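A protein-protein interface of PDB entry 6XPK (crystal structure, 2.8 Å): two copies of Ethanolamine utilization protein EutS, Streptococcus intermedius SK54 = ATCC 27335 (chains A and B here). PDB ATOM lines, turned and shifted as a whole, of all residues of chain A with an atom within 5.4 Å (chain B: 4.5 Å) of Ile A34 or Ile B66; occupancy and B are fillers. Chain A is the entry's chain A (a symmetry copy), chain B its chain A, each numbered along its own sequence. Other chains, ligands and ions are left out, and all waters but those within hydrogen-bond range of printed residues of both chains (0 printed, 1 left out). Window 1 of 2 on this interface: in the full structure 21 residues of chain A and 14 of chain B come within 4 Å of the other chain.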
ATOM      1  N   LEU A  30       9.348  14.396   9.459  1.00  0.00           N
ATOM      2  CA  LEU A  30       9.449  13.280  10.437  1.00  0.00           C
ATOM      3  C   LEU A  30      10.607  13.552  11.405  1.00  0.00           C
ATOM      4  O   LEU A  30      11.670  14.011  10.945  1.00  0.00           O
ATOM      5  CB  LEU A  30       9.662  11.964   9.680  1.00  0.00           C
ATOM      6  CG  LEU A  30       9.438  10.689  10.491  1.00  0.00           C
ATOM      7  CD1 LEU A  30       7.952  10.412  10.673  1.00  0.00           C
ATOM      8  CD2 LEU A  30      10.118   9.504   9.826  1.00  0.00           C
ATOM      9  N   HIS A  32      11.115  10.963  14.417  1.00  0.00           N
ATOM     10  CA  HIS A  32      10.508   9.786  15.092  1.00  0.00           C
ATOM     11  C   HIS A  32      11.574   9.011  15.872  1.00  0.00           C
ATOM     12  O   HIS A  32      12.744   9.022  15.447  1.00  0.00           O
ATOM     13  CB  HIS A  32       9.810   8.909  14.045  1.00  0.00           C
ATOM     14  CG  HIS A  32       9.129   7.709  14.611  1.00  0.00           C
ATOM     15  ND1 HIS A  32       7.796   7.717  14.966  1.00  0.00           N
ATOM     16  CD2 HIS A  32       9.587   6.468  14.875  1.00  0.00           C
ATOM     17  CE1 HIS A  32       7.462   6.530  15.428  1.00  0.00           C
ATOM     18  NE2 HIS A  32       8.543   5.747  15.383  1.00  0.00           N
ATOM     19  N   VAL A  33      11.165   8.359  16.966  1.00  0.00           N
ATOM     20  CA  VAL A  33      12.019   7.461  17.802  1.00  0.00           C
ATOM     21  C   VAL A  33      11.317   6.103  17.918  1.00  0.00           C
ATOM     22  O   VAL A  33      10.118   6.085  18.257  1.00  0.00           O
ATOM     23  CB  VAL A  33      12.320   8.072  19.187  1.00  0.00           C
ATOM     24  CG1 VAL A  33      11.103   8.747  19.801  1.00  0.00           C
ATOM     25  CG2 VAL A  33      12.904   7.047  20.149  1.00  0.00           C
ATOM     26  N   ILE A  34      12.041   5.018  17.630  1.00  0.00           N
ATOM     27  CA  ILE A  34      11.590   3.611  17.849  1.00  0.00           C
ATOM     28  C   ILE A  34      12.240   3.119  19.148  1.00  0.00           C
ATOM     29  O   ILE A  34      13.434   2.766  19.112  1.00  0.00           O
ATOM     30  CB  ILE A  34      11.937   2.716  16.639  1.00  0.00           C
ATOM     31  CG1 ILE A  34      11.560   3.387  15.313  1.00  0.00           C
ATOM     32  CG2 ILE A  34      11.292   1.345  16.783  1.00  0.00           C
ATOM     33  CD1 ILE A  34      11.841   2.548  14.087  1.00  0.00           C
ATOM     34  N   ALA A  35      11.480   3.123  20.250  1.00  0.00           N
ATOM     35  CA  ALA A  35      11.957   2.842  21.627  1.00  0.00           C
ATOM     36  C   ALA A  35      12.477   1.404  21.728  1.00  0.00           C
ATOM     37  O   ALA A  35      13.598   1.221  22.245  1.00  0.00           O
ATOM     38  CB  ALA A  35      10.848   3.097  22.619  1.00  0.00           C
ATOM     39  N   ALA A  36      11.698   0.428  21.248  1.00  0.00           N
ATOM     40  CA  ALA A  36      12.005  -1.022  21.306  1.00  0.00           C
ATOM     41  C   ALA A  36      11.943  -1.633  19.905  1.00  0.00           C
ATOM     42  O   ALA A  36      10.949  -2.261  19.546  1.00  0.00           O
ATOM     43  CB  ALA A  36      11.049  -1.704  22.252  1.00  0.00           C
ATOM     44  N   PRO A  37      12.993  -1.462  19.067  1.00  0.00           N
ATOM     45  CA  PRO A  37      13.071  -2.135  17.767  1.00  0.00           C
ATOM     46  C   PRO A  37      13.208  -3.664  17.877  1.00  0.00           C
ATOM     47  O   PRO A  37      13.481  -4.151  18.961  1.00  0.00           O
ATOM     48  CB  PRO A  37      14.326  -1.545  17.103  1.00  0.00           C
ATOM     49  CG  PRO A  37      14.642  -0.293  17.899  1.00  0.00           C
ATOM     50  CD  PRO A  37      14.137  -0.568  19.299  1.00  0.00           C
ATOM     51  N   VAL A  41      14.651  -5.205  12.270  1.00  0.00           N
ATOM     52  CA  VAL A  41      14.901  -3.733  12.182  1.00  0.00           C
ATOM     53  C   VAL A  41      16.387  -3.460  12.450  1.00  0.00           C
ATOM     54  O   VAL A  41      16.984  -2.667  11.696  1.00  0.00           O
ATOM     55  CB  VAL A  41      13.995  -2.948  13.150  1.00  0.00           C
ATOM     56  CG1 VAL A  41      14.414  -1.491  13.273  1.00  0.00           C
ATOM     57  CG2 VAL A  41      12.529  -3.055  12.752  1.00  0.00           C
ATOM     58  N   GLY A  51      19.322  -0.630  22.039  1.00  0.00           N
ATOM     59  CA  GLY A  51      18.930   0.791  22.135  1.00  0.00           C
ATOM     60  C   GLY A  51      17.831   1.164  21.154  1.00  0.00           C
ATOM     61  O   GLY A  51      17.432   0.300  20.346  1.00  0.00           O
ATOM     62  N   ALA A  52      17.367   2.416  21.228  1.00  0.00           N
ATOM     63  CA  ALA A  52      16.326   3.006  20.352  1.00  0.00           C
ATOM     64  C   ALA A  52      16.950   3.422  19.016  1.00  0.00           C
ATOM     65  O   ALA A  52      18.192   3.381  18.904  1.00  0.00           O
ATOM     66  CB  ALA A  52      15.676   4.183  21.039  1.00  0.00           C
ATOM     67  N   ILE A  53      16.111   3.804  18.049  1.00  0.00           N
ATOM     68  CA  ILE A  53      16.522   4.314  16.706  1.00  0.00           C
ATOM     69  C   ILE A  53      15.759   5.615  16.430  1.00  0.00           C
ATOM     70  O   ILE A  53      14.513   5.577  16.433  1.00  0.00           O
ATOM     71  CB  ILE A  53      16.280   3.251  15.614  1.00  0.00           C
ATOM     72  CG1 ILE A  53      17.278   2.095  15.726  1.00  0.00           C
ATOM     73  CG2 ILE A  53      16.305   3.873  14.224  1.00  0.00           C
ATOM     74  CD1 ILE A  53      16.802   0.810  15.091  1.00  0.00           C
ATOM     75  N   GLY A  54      16.487   6.714  16.216  1.00  0.00           N
ATOM     76  CA  GLY A  54      15.931   8.022  15.816  1.00  0.00           C
ATOM     77  C   GLY A  54      15.911   8.165  14.305  1.00  0.00           C
ATOM     78  O   GLY A  54      16.980   7.995  13.691  1.00  0.00           O
ATOM     79  N   VAL A  55      14.740   8.453  13.727  1.00  0.00           N
ATOM     80  CA  VAL A  55      14.527   8.614  12.258  1.00  0.00           C
ATOM     81  C   VAL A  55      14.091  10.059  11.993  1.00  0.00           C
ATOM     82  O   VAL A  55      13.211  10.552  12.726  1.00  0.00           O
ATOM     83  CB  VAL A  55      13.488   7.608  11.723  1.00  0.00           C
ATOM     84  CG1 VAL A  55      13.413   7.628  10.204  1.00  0.00           C
ATOM     85  CG2 VAL A  55      13.754   6.195  12.223  1.00  0.00           C
ATOM     86  N   SER A 123       7.240   5.026  18.811  1.00  0.00           N
ATOM     87  CA  SER A 123       6.699   3.675  18.504  1.00  0.00           C
ATOM     88  C   SER A 123       7.605   2.602  19.122  1.00  0.00           C
ATOM     89  O   SER A 123       8.582   2.909  19.808  1.00  0.00           O
ATOM     90  CB  SER A 123       6.539   3.471  17.019  1.00  0.00           C
ATOM     91  OG  SER A 123       7.794   3.235  16.398  1.00  0.00           O
ATOM     92  OXT SER A 123       7.378   1.405  18.950  1.00  0.00           O
ATOM     93  N   THR B  63      11.037   5.074   6.136  1.00  0.00           N
ATOM     94  CA  THR B  63       9.967   4.804   7.137  1.00  0.00           C
ATOM     95  C   THR B  63       9.433   3.372   6.984  1.00  0.00           C
ATOM     96  O   THR B  63       8.515   3.010   7.744  1.00  0.00           O
ATOM     97  CB  THR B  63       8.858   5.862   7.053  1.00  0.00           C
ATOM     98  OG1 THR B  63       8.314   5.887   5.736  1.00  0.00           O
ATOM     99  CG2 THR B  63       9.351   7.253   7.376  1.00  0.00           C
ATOM    100  N   ALA B  64       9.986   2.590   6.047  1.00  0.00           N
ATOM    101  CA  ALA B  64       9.807   1.121   5.946  1.00  0.00           C
ATOM    102  C   ALA B  64      10.280   0.461   7.247  1.00  0.00           C
ATOM    103  O   ALA B  64       9.732  -0.599   7.608  1.00  0.00           O
ATOM    104  CB  ALA B  64      10.566   0.586   4.755  1.00  0.00           C
ATOM    105  N   ILE B  65      11.261   1.074   7.919  1.00  0.00           N
ATOM    106  CA  ILE B  65      11.840   0.601   9.212  1.00  0.00           C
ATOM    107  C   ILE B  65      10.781   0.736  10.317  1.00  0.00           C
ATOM    108  O   ILE B  65      10.723  -0.156  11.186  1.00  0.00           O
ATOM    109  CB  ILE B  65      13.145   1.363   9.537  1.00  0.00           C
ATOM    110  CG1 ILE B  65      14.192   0.442  10.166  1.00  0.00           C
ATOM    111  CG2 ILE B  65      12.887   2.594  10.396  1.00  0.00           C
ATOM    112  CD1 ILE B  65      14.896  -0.455   9.172  1.00  0.00           C
ATOM    113  N   ILE B  66       9.975   1.806  10.279  1.00  0.00           N
ATOM    114  CA  ILE B  66       8.915   2.111  11.289  1.00  0.00           C
ATOM    115  C   ILE B  66       7.713   1.191  11.033  1.00  0.00           C
ATOM    116  O   ILE B  66       7.137   0.693  12.018  1.00  0.00           O
ATOM    117  CB  ILE B  66       8.519   3.603  11.259  1.00  0.00           C
ATOM    118  CG1 ILE B  66       9.728   4.521  11.470  1.00  0.00           C
ATOM    119  CG2 ILE B  66       7.418   3.889  12.274  1.00  0.00           C
ATOM    120  CD1 ILE B  66       9.430   5.995  11.302  1.00  0.00           C
ATOM    121  N   ALA B  67       7.347   0.992   9.762  1.00  0.00           N
ATOM    122  CA  ALA B  67       6.240   0.111   9.319  1.00  0.00           C
ATOM    123  C   ALA B  67       6.537  -1.338   9.727  1.00  0.00           C
ATOM    124  O   ALA B  67       5.623  -2.001  10.253  1.00  0.00           O
ATOM    125  CB  ALA B  67       6.043   0.236   7.827  1.00  0.00           C
ATOM    126  N   ALA B  68       7.771  -1.798   9.495  1.00  0.00           N
ATOM    127  CA  ALA B  68       8.267  -3.152   9.845  1.00  0.00           C
ATOM    128  C   ALA B  68       8.153  -3.381  11.358  1.00  0.00           C
ATOM    129  O   ALA B  68       7.816  -4.513  11.759  1.00  0.00           O
ATOM    130  CB  ALA B  68       9.690  -3.319   9.374  1.00  0.00           C
ATOM    131  N   ASP B  69       8.429  -2.343  12.156  1.00  0.00           N
ATOM    132  CA  ASP B  69       8.376  -2.368  13.644  1.00  0.00           C
ATOM    133  C   ASP B  69       6.947  -2.683  14.102  1.00  0.00           C
ATOM    134  O   ASP B  69       6.789  -3.556  14.978  1.00  0.00           O
ATOM    135  CB  ASP B  69       8.862  -1.040  14.232  1.00  0.00           C
ATOM    136  CG  ASP B  69       9.013  -1.050  15.743  1.00  0.00           C
ATOM    137  OD1 ASP B  69       9.936  -1.724  16.233  1.00  0.00           O
ATOM    138  OD2 ASP B  69       8.203  -0.382  16.418  1.00  0.00           O
ATOM    139  N   ILE B  70       5.952  -2.001  13.523  1.00  0.00           N
ATOM    140  CA  ILE B  70       4.507  -2.114  13.895  1.00  0.00           C
ATOM    141  C   ILE B  70       3.974  -3.477  13.431  1.00  0.00           C
ATOM    142  O   ILE B  70       3.180  -4.079  14.178  1.00  0.00           O
ATOM    143  CB  ILE B  70       3.691  -0.939  13.314  1.00  0.00           C
ATOM    144  CG1 ILE B  70       4.194   0.411  13.833  1.00  0.00           C
ATOM    145  CG2 ILE B  70       2.204  -1.121  13.588  1.00  0.00           C
ATOM    146  CD1 ILE B  70       3.730   1.593  13.015  1.00  0.00           C
ATOM    147  N   PHE B 109       0.394   5.521  11.024  1.00  0.00           N
ATOM    148  CA  PHE B 109       1.012   6.409  10.002  1.00  0.00           C
ATOM    149  C   PHE B 109       0.047   7.548   9.648  1.00  0.00           C
ATOM    150  O   PHE B 109       0.512   8.696   9.501  1.00  0.00           O
ATOM    151  CB  PHE B 109       1.424   5.610   8.762  1.00  0.00           C
ATOM    152  CG  PHE B 109       2.794   4.980   8.839  1.00  0.00           C
ATOM    153  CD1 PHE B 109       3.036   3.896   9.669  1.00  0.00           C
ATOM    154  CD2 PHE B 109       3.841   5.467   8.072  1.00  0.00           C
ATOM    155  CE1 PHE B 109       4.296   3.318   9.733  1.00  0.00           C
ATOM    156  CE2 PHE B 109       5.101   4.889   8.138  1.00  0.00           C
ATOM    157  CZ  PHE B 109       5.326   3.815   8.968  1.00  0.00           C
ATOM    158  N   LEU B 113       1.756   9.960  12.356  1.00  0.00           N
ATOM    159  CA  LEU B 113       2.857  10.430  11.468  1.00  0.00           C
ATOM    160  C   LEU B 113       2.306  11.302  10.330  1.00  0.00           C
ATOM    161  O   LEU B 113       3.126  11.807   9.536  1.00  0.00           O
ATOM    162  CB  LEU B 113       3.614   9.217  10.916  1.00  0.00           C
ATOM    163  CG  LEU B 113       4.088   8.198  11.952  1.00  0.00           C
ATOM    164  CD1 LEU B 113       4.922   7.108  11.295  1.00  0.00           C
ATOM    165  CD2 LEU B 113       4.879   8.866  13.067  1.00  0.00           C
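Ile A34 touches just these residues of chain B: Ile B65 (3.8 Å), Ile B66 (3.9 Å) and Asp B69 (3.4 Å).
Ile B66 touches three residues of chain A.
Printed residues of chain B within 4 Å of Ser A123: Asp B69.
Of the printed residues of chain A, Thr B63 touches Leu A30 (3.4 Å).
Of the printed residues of chain B, Leu A30 touches Thr B63 and Ile B66.
Printed residues of chain A within 4 Å of Ile B65: Ile A34 and Val A41.
Printed residues of chain B within 4 Å of Ala A36: Asp B69 (3.5 Å).
Ala B67 touches none of the printed residues of chain A.
Ala B68 touches none of the printed residues of chain A.
The backbone NH (N) of Ile A34 lies within hydrogen-bond range of the backbone carbonyl oxygen (O) of Ile A53 (2.8 Å).
NE2 of His A32 lies within hydrogen-bond range of OG of Ser A123.
O of Ser A123 is in hydrogen-bond range of N of Ala A35.
The backbone NH (N) of Ser A123 is in hydrogen-bond range of the backbone carbonyl oxygen (O) of Val A33 (3.1 Å).
O of His A32 lies within hydrogen-bond range of N of Val A55.
Of the 14 printed residues of chain A, 7 touch a printed residue of chain B.
Printed residues of chain A that touch a printed residue of chain B: Leu A30, His A32, Ile A34, Ala A36, Pro A37, Val A41 and Ser A123.
Hydrophobic or aromatic side chains of chain A that line the printed part of chain B: Leu A30, His A32, Ile A34 and Val A41.
Printed residues of chain B that touch a printed residue of chain A: Thr B63, Ile B65, Ile B66, Asp B69 and Leu B113.
Hydrophobic or aromatic side chains of chain B that line the printed part of chain A: Ile B65, Ile B66 and Leu B113.
Among the printed residues, pairs that only touch across the chains: Ile A34 with Asp B69 (3.4 Å), Leu A30 with Thr B63 (3.4 Å), Ala A36 with Asp B69 (3.5 Å), Pro A37 with Asp B69 (3.5 Å), His A32 with Ile B66 (3.6 Å), His A32 with Leu B113 (3.7 Å), Val A41 with Ile B65 (3.7 Å), Ile A34 with Ile B65 (3.8 Å), Leu A30 with Ile B66 (3.9 Å) and Ile A34 with Ile B66 (3.9 Å).
No position is printed for both chains.
The chain-end carboxylate of Ser A123 sits close to the side-chain carboxylate of Asp B69 (3.2 Å).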
